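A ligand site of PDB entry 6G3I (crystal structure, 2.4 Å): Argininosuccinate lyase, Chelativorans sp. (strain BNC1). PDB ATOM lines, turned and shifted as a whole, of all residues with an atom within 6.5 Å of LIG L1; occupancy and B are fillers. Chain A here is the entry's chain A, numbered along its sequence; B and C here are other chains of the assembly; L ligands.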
ATOM      1  N   GLY A 278      28.304  18.076  11.594  1.00  0.00           N
ATOM      2  CA  GLY A 278      27.320  18.411  10.586  1.00  0.00           C
ATOM      3  C   GLY A 278      27.984  18.935   9.338  1.00  0.00           C
ATOM      4  O   GLY A 278      29.187  18.714   9.141  1.00  0.00           O
ATOM      5  N   THR A 279      27.232  19.626   8.487  1.00  0.00           N
ATOM      6  CA  THR A 279      27.809  20.215   7.284  1.00  0.00           C
ATOM      7  C   THR A 279      26.995  21.438   6.901  1.00  0.00           C
ATOM      8  O   THR A 279      26.033  21.814   7.585  1.00  0.00           O
ATOM      9  CB  THR A 279      27.858  19.189   6.137  1.00  0.00           C
ATOM     10  OG1 THR A 279      28.485  19.785   4.985  1.00  0.00           O
ATOM     11  CG2 THR A 279      26.458  18.716   5.769  1.00  0.00           C
ATOM     12  N   SER A 280      27.376  22.068   5.799  1.00  0.00           N
ATOM     13  CA  SER A 280      26.777  23.313   5.349  1.00  0.00           C
ATOM     14  C   SER A 280      25.739  23.050   4.263  1.00  0.00           C
ATOM     15  O   SER A 280      25.851  22.107   3.473  1.00  0.00           O
ATOM     16  CB  SER A 280      27.849  24.256   4.806  1.00  0.00           C
ATOM     17  OG  SER A 280      27.271  25.381   4.162  1.00  0.00           O
ATOM     18  N   SER A 281      24.711  23.892   4.237  1.00  0.00           N
ATOM     19  CA  SER A 281      23.709  23.849   3.174  1.00  0.00           C
ATOM     20  C   SER A 281      24.200  24.471   1.881  1.00  0.00           C
ATOM     21  O   SER A 281      23.493  24.404   0.873  1.00  0.00           O
ATOM     22  CB  SER A 281      22.427  24.560   3.636  1.00  0.00           C
ATOM     23  OG  SER A 281      22.626  25.969   3.694  1.00  0.00           O
ATOM     24  N   ILE A 282      25.399  25.060   1.872  1.00  0.00           N
ATOM     25  CA  ILE A 282      25.915  25.768   0.718  1.00  0.00           C
ATOM     26  C   ILE A 282      27.323  25.275   0.369  1.00  0.00           C
ATOM     27  O   ILE A 282      27.664  25.128  -0.805  1.00  0.00           O
ATOM     28  CB  ILE A 282      25.911  27.296   0.953  1.00  0.00           C
ATOM     29  CG1 ILE A 282      26.559  28.027  -0.221  1.00  0.00           C
ATOM     30  CG2 ILE A 282      26.616  27.636   2.263  1.00  0.00           C
ATOM     31  CD1 ILE A 282      26.385  29.535  -0.185  1.00  0.00           C
ATOM     32  N   MET A 283      28.130  25.007   1.392  1.00  0.00           N
ATOM     33  CA  MET A 283      29.511  24.617   1.187  1.00  0.00           C
ATOM     34  C   MET A 283      29.653  23.109   1.352  1.00  0.00           C
ATOM     35  O   MET A 283      29.573  22.614   2.489  1.00  0.00           O
ATOM     36  CB  MET A 283      30.425  25.340   2.177  1.00  0.00           C
ATOM     37  CG  MET A 283      30.557  26.843   1.909  1.00  0.00           C
ATOM     38  SD  MET A 283      31.380  27.744   3.231  1.00  0.00           S
ATOM     39  CE  MET A 283      30.231  27.526   4.582  1.00  0.00           C
ATOM     40  N   LYS A 286      32.272  21.191   4.063  1.00  0.00           N
ATOM     41  CA  LYS A 286      32.294  21.408   5.505  1.00  0.00           C
ATOM     42  C   LYS A 286      32.044  20.131   6.281  1.00  0.00           C
ATOM     43  O   LYS A 286      31.120  19.370   5.991  1.00  0.00           O
ATOM     44  CB  LYS A 286      31.242  22.451   5.894  1.00  0.00           C
ATOM     45  CG  LYS A 286      31.637  23.894   5.606  1.00  0.00           C
ATOM     46  CD  LYS A 286      32.954  24.269   6.267  1.00  0.00           C
ATOM     47  CE  LYS A 286      32.910  25.644   6.905  1.00  0.00           C
ATOM     48  NZ  LYS A 286      32.094  25.636   8.129  1.00  0.00           N
ATOM     49  N   ASN A 288      31.399  20.243  10.056  1.00  0.00           N
ATOM     50  CA  ASN A 288      31.316  21.297  11.058  1.00  0.00           C
ATOM     51  C   ASN A 288      31.191  20.755  12.472  1.00  0.00           C
ATOM     52  O   ASN A 288      30.465  19.783  12.717  1.00  0.00           O
ATOM     53  CB  ASN A 288      30.103  22.181  10.770  1.00  0.00           C
ATOM     54  CG  ASN A 288      30.321  23.049   9.561  1.00  0.00           C
ATOM     55  OD1 ASN A 288      31.452  23.411   9.250  1.00  0.00           O
ATOM     56  ND2 ASN A 288      29.247  23.382   8.866  1.00  0.00           N
ATOM     57  N   ASP A 290      29.466  21.171  15.095  1.00  0.00           N
ATOM     58  CA  ASP A 290      28.222  21.632  15.711  1.00  0.00           C
ATOM     59  C   ASP A 290      28.083  21.124  17.136  1.00  0.00           C
ATOM     60  O   ASP A 290      27.598  21.849  18.011  1.00  0.00           O
ATOM     61  CB  ASP A 290      27.029  21.181  14.870  1.00  0.00           C
ATOM     62  CG  ASP A 290      27.003  21.815  13.490  1.00  0.00           C
ATOM     63  OD1 ASP A 290      27.591  22.903  13.335  1.00  0.00           O
ATOM     64  OD2 ASP A 290      26.400  21.231  12.569  1.00  0.00           O
ATOM     65  N   LEU B  89      16.451  23.386   6.785  1.00  0.00           N
ATOM     66  CA  LEU B  89      16.619  22.256   5.884  1.00  0.00           C
ATOM     67  C   LEU B  89      15.421  21.323   5.918  1.00  0.00           C
ATOM     68  O   LEU B  89      14.979  20.849   4.862  1.00  0.00           O
ATOM     69  CB  LEU B  89      17.923  21.510   6.191  1.00  0.00           C
ATOM     70  CG  LEU B  89      19.186  22.190   5.636  1.00  0.00           C
ATOM     71  CD1 LEU B  89      20.441  21.469   6.115  1.00  0.00           C
ATOM     72  CD2 LEU B  89      19.180  22.270   4.111  1.00  0.00           C
ATOM     73  N   HIS B 107      17.445  28.428  -2.581  1.00  0.00           N
ATOM     74  CA  HIS B 107      18.643  28.645  -1.778  1.00  0.00           C
ATOM     75  C   HIS B 107      19.811  29.164  -2.612  1.00  0.00           C
ATOM     76  O   HIS B 107      20.922  29.293  -2.070  1.00  0.00           O
ATOM     77  CB  HIS B 107      19.040  27.343  -1.087  1.00  0.00           C
ATOM     78  CG  HIS B 107      19.716  27.542   0.243  1.00  0.00           C
ATOM     79  ND1 HIS B 107      19.309  28.500   1.139  1.00  0.00           N
ATOM     80  CD2 HIS B 107      20.743  26.892   0.822  1.00  0.00           C
ATOM     81  CE1 HIS B 107      20.066  28.443   2.221  1.00  0.00           C
ATOM     82  NE2 HIS B 107      20.954  27.473   2.053  1.00  0.00           N
ATOM     83  N   ARG B 110      22.587  31.929  -1.264  1.00  0.00           N
ATOM     84  CA  ARG B 110      22.094  32.134   0.094  1.00  0.00           C
ATOM     85  C   ARG B 110      22.575  30.991   0.971  1.00  0.00           C
ATOM     86  O   ARG B 110      22.909  29.900   0.496  1.00  0.00           O
ATOM     87  CB  ARG B 110      20.568  32.248   0.107  1.00  0.00           C
ATOM     88  CG  ARG B 110      19.947  32.364   1.485  1.00  0.00           C
ATOM     89  CD  ARG B 110      18.436  32.519   1.399  1.00  0.00           C
ATOM     90  NE  ARG B 110      17.763  31.234   1.277  1.00  0.00           N
ATOM     91  CZ  ARG B 110      16.447  31.070   1.318  1.00  0.00           C
ATOM     92  NH1 ARG B 110      15.660  32.127   1.472  1.00  0.00           N
ATOM     93  NH2 ARG B 110      15.921  29.859   1.214  1.00  0.00           N
ATOM     94  N   SER B 111      22.594  31.257   2.281  1.00  0.00           N
ATOM     95  CA  SER B 111      23.057  30.301   3.271  1.00  0.00           C
ATOM     96  C   SER B 111      22.084  30.299   4.434  1.00  0.00           C
ATOM     97  O   SER B 111      21.237  31.188   4.571  1.00  0.00           O
ATOM     98  CB  SER B 111      24.470  30.656   3.765  1.00  0.00           C
ATOM     99  OG  SER B 111      24.879  29.813   4.828  1.00  0.00           O
ATOM    100  N   ARG B 112      22.192  29.271   5.293  1.00  0.00           N
ATOM    101  CA  ARG B 112      21.494  29.324   6.562  1.00  0.00           C
ATOM    102  C   ARG B 112      22.040  30.445   7.437  1.00  0.00           C
ATOM    103  O   ARG B 112      21.308  30.987   8.279  1.00  0.00           O
ATOM    104  CB  ARG B 112      21.616  27.978   7.284  1.00  0.00           C
ATOM    105  CG  ARG B 112      20.579  26.949   6.866  1.00  0.00           C
ATOM    106  CD  ARG B 112      20.714  25.644   7.645  1.00  0.00           C
ATOM    107  NE  ARG B 112      22.087  25.157   7.678  1.00  0.00           N
ATOM    108  CZ  ARG B 112      22.483  24.070   8.336  1.00  0.00           C
ATOM    109  NH1 ARG B 112      21.605  23.338   9.024  1.00  0.00           N
ATOM    110  NH2 ARG B 112      23.758  23.708   8.313  1.00  0.00           N
ATOM    111  N   ASN B 113      23.302  30.831   7.232  1.00  0.00           N
ATOM    112  CA  ASN B 113      23.956  31.786   8.111  1.00  0.00           C
ATOM    113  C   ASN B 113      23.346  33.177   7.977  1.00  0.00           C
ATOM    114  O   ASN B 113      22.994  33.806   8.991  1.00  0.00           O
ATOM    115  CB  ASN B 113      25.457  31.818   7.803  1.00  0.00           C
ATOM    116  CG  ASN B 113      26.143  30.523   8.212  1.00  0.00           C
ATOM    117  OD1 ASN B 113      25.506  29.599   8.685  1.00  0.00           O
ATOM    118  ND2 ASN B 113      27.458  30.465   8.007  1.00  0.00           N
ATOM    119  N   ALA B 201      25.452  35.449   2.283  1.00  0.00           N
ATOM    120  CA  ALA B 201      25.502  34.004   2.049  1.00  0.00           C
ATOM    121  C   ALA B 201      26.238  33.378   3.232  1.00  0.00           C
ATOM    122  O   ALA B 201      25.910  33.706   4.392  1.00  0.00           O
ATOM    123  CB  ALA B 201      26.113  33.743   0.679  1.00  0.00           C
ATOM    124  N   ALA B 202      27.212  32.494   3.025  1.00  0.00           N
ATOM    125  CA  ALA B 202      27.901  31.849   4.139  1.00  0.00           C
ATOM    126  C   ALA B 202      28.705  32.842   4.960  1.00  0.00           C
ATOM    127  O   ALA B 202      28.795  32.689   6.184  1.00  0.00           O
ATOM    128  CB  ALA B 202      28.805  30.729   3.618  1.00  0.00           C
ATOM    129  N   TYR B 320      31.179  33.733  11.635  1.00  0.00           N
ATOM    130  CA  TYR B 320      29.928  33.073  11.973  1.00  0.00           C
ATOM    131  C   TYR B 320      30.242  31.922  12.932  1.00  0.00           C
ATOM    132  O   TYR B 320      31.254  31.234  12.779  1.00  0.00           O
ATOM    133  CB  TYR B 320      29.224  32.541  10.723  1.00  0.00           C
ATOM    134  CG  TYR B 320      28.061  31.641  11.081  1.00  0.00           C
ATOM    135  CD1 TYR B 320      26.793  32.169  11.279  1.00  0.00           C
ATOM    136  CD2 TYR B 320      28.249  30.284  11.263  1.00  0.00           C
ATOM    137  CE1 TYR B 320      25.733  31.348  11.630  1.00  0.00           C
ATOM    138  CE2 TYR B 320      27.202  29.464  11.609  1.00  0.00           C
ATOM    139  CZ  TYR B 320      25.946  30.000  11.798  1.00  0.00           C
ATOM    140  OH  TYR B 320      24.899  29.180  12.144  1.00  0.00           O
ATOM    141  N   ALA B 322      28.143  29.008  15.798  1.00  0.00           N
ATOM    142  CA  ALA B 322      26.946  28.479  16.443  1.00  0.00           C
ATOM    143  C   ALA B 322      27.061  28.474  17.954  1.00  0.00           C
ATOM    144  O   ALA B 322      26.156  27.981  18.630  1.00  0.00           O
ATOM    145  CB  ALA B 322      26.659  27.068  15.927  1.00  0.00           C
ATOM    146  N   THR C 158      34.251  29.824   8.975  1.00  0.00           N
ATOM    147  CA  THR C 158      33.043  29.768   9.779  1.00  0.00           C
ATOM    148  C   THR C 158      33.151  28.549  10.669  1.00  0.00           C
ATOM    149  O   THR C 158      33.519  27.471  10.214  1.00  0.00           O
ATOM    150  CB  THR C 158      31.765  29.696   8.937  1.00  0.00           C
ATOM    151  OG1 THR C 158      31.669  28.404   8.320  1.00  0.00           O
ATOM    152  CG2 THR C 158      31.760  30.782   7.856  1.00  0.00           C
ATOM    153  N   GLN C 159      32.844  28.731  11.950  1.00  0.00           N
ATOM    154  CA  GLN C 159      32.983  27.657  12.934  1.00  0.00           C
ATOM    155  C   GLN C 159      34.400  27.097  12.976  1.00  0.00           C
ATOM    156  O   GLN C 159      34.601  25.909  13.223  1.00  0.00           O
ATOM    157  CB  GLN C 159      31.993  26.524  12.661  1.00  0.00           C
ATOM    158  CG  GLN C 159      30.553  26.961  12.531  1.00  0.00           C
ATOM    159  CD  GLN C 159      29.606  25.784  12.349  1.00  0.00           C
ATOM    160  OE1 GLN C 159      29.396  25.325  11.229  1.00  0.00           O
ATOM    161  NE2 GLN C 159      29.045  25.296  13.445  1.00  0.00           N
ATOM    162  N   ALA C 163      36.004  28.042   4.911  1.00  0.00           N
ATOM    163  CA  ALA C 163      34.691  28.224   4.299  1.00  0.00           C
ATOM    164  C   ALA C 163      34.810  28.585   2.819  1.00  0.00           C
ATOM    165  O   ALA C 163      34.442  27.772   1.972  1.00  0.00           O
ATOM    166  CB  ALA C 163      33.909  29.294   5.064  1.00  0.00           C
HETATM  167  O1  LIG L   1      24.576  27.436   5.005  1.00  0.00           O
HETATM  168  C1  LIG L   1      25.215  26.824   5.971  1.00  0.00           C
HETATM  169  O2  LIG L   1      24.783  25.810   6.552  1.00  0.00           O
HETATM  170  C2  LIG L   1      26.509  27.314   6.443  1.00  0.00           C
HETATM  171  C3  LIG L   1      27.088  26.521   7.599  1.00  0.00           C
HETATM  172  C4  LIG L   1      28.569  26.754   7.753  1.00  0.00           C
HETATM  173  O3  LIG L   1      29.243  25.733   7.570  1.00  0.00           O
HETATM  174  O4  LIG L   1      29.003  27.865   8.057  1.00  0.00           O
HETATM  175  N1  LIG L   1      26.325  26.898   8.875  1.00  0.00           N
HETATM  176  C5  LIG L   1      26.831  26.188  10.136  1.00  0.00           C
HETATM  177  C6  LIG L   1      25.952  25.053  10.640  1.00  0.00           C
HETATM  178  N2  LIG L   1      26.589  23.692  10.263  1.00  0.00           N
HETATM  179  O1  LG2 L   2      24.166  24.190  15.150  1.00  0.00           O
HETATM  180  C1  LG2 L   2      23.699  24.021  14.001  1.00  0.00           C
HETATM  181  O2  LG2 L   2      23.337  22.885  13.628  1.00  0.00           O
HETATM  182  C2  LG2 L   2      23.544  25.169  13.031  1.00  0.00           C
HETATM  183  C3  LG2 L   2      22.379  25.330  12.466  1.00  0.00           C
HETATM  184  C4  LG2 L   2      22.231  26.468  11.465  1.00  0.00           C
HETATM  185  O3  LG2 L   2      21.195  27.176  11.428  1.00  0.00           O
HETATM  186  O4  LG2 L   2      23.188  26.669  10.666  1.00  0.00           O
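Ile 282 touches LIG L1 (CG2 to O1, 3.4 Å).
CE of Met 283 touches O3 of LIG L1, 3.6 Å away.
Tyr 320 of chain B touches LIG L1.
Hydrophobic or aromatic side chains that line LIG L1: Ile 282, Met 283 and Tyr 320 of chain B.
The nearest printed residue that does not touch LIG L1 is His 107 of chain B (4.7 Å).
OG of Ser 111 of chain B lies within hydrogen-bond range of N of Asn 113 of chain B (3.0 Å).
The side-chain amide oxygen (OD1) of Asn 288 is in hydrogen-bond range of the side-chain amino group (NZ) of Lys 286, 2.6 Å away.
NH2 of Arg 112 of chain B lies within hydrogen-bond range of O of Thr 279 (3.0 Å).
The side-chain hydroxyl (OG) of Ser 280 lies within hydrogen-bond range of the backbone NH (N) of Met 283 (2.9 Å).
The side-chain hydroxyl (OG) of Ser 280 sits at hydrogen-bond distance from the backbone NH (N) of Ile 282 (3.0 Å).
The side-chain hydroxyl of Thr 158 of chain C is in hydrogen-bond range of the side-chain amino group of Lys 286, at 2.8 Å.
The backbone carbonyl oxygen (O) of Gly 278 sits at hydrogen-bond distance from the backbone NH (N) of Asn 288, at 2.8 Å.
The side-chain amide nitrogen (NE2) of Gln 159 of chain C lies within hydrogen-bond range of the side-chain carboxylate (OD1) of Asp 290.
N of Ser 281 is in hydrogen-bond range of O2 of LIG L1, 3.0 Å away.
The side-chain carboxylate (OD1) of Asp 290 is in salt-bridge range of a nitrogen (N2) of LIG L1, at 3.3 Å.
NH2 of Arg 112 of chain B is in salt-bridge range of O2 of LIG L1, at 2.9 Å.
An oxygen (O4) of LG2 L2 sits at hydrogen-bond distance from the side-chain hydroxyl of Tyr 320 of chain B (3.4 Å).
The side-chain hydroxyl (OG) of Ser 281 is in hydrogen-bond range of an oxygen (O1) of LIG L1.
The side-chain amide oxygen of Gln 159 of chain C lies close to a nitrogen (N2) of LIG L1 (3.4 Å).
The backbone NH of Arg 112 of chain B is in hydrogen-bond range of an oxygen (O1) of LIG L1, at 3.0 Å.
O4 of LIG L1 sits at hydrogen-bond distance from OG1 of Thr 158 of chain C.
The guanidinium group (NE) of Arg 112 of chain B is in salt-bridge range of an oxygen (O4) of LG2 L2 (3.5 Å).
The side-chain amide oxygen of Asn 113 of chain B is in hydrogen-bond range of a nitrogen (N1) of LIG L1.
An oxygen (O1) of LIG L1 is in hydrogen-bond range of the side-chain hydroxyl of Ser 111 of chain B (2.4 Å).
The side-chain amide nitrogen (ND2) of Asn 288 is in hydrogen-bond range of an oxygen (O3) of LIG L1, at 2.7 Å.
The side-chain hydroxyl of Ser 280 sits close to an oxygen (O2) of LIG L1, 3.5 Å away.
O of Thr 279 sits at hydrogen-bond distance from N2 of LIG L1.
The side-chain amino group (NZ) of Lys 286 lies within salt-bridge range of an oxygen (O3) of LIG L1, at 2.9 Å.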
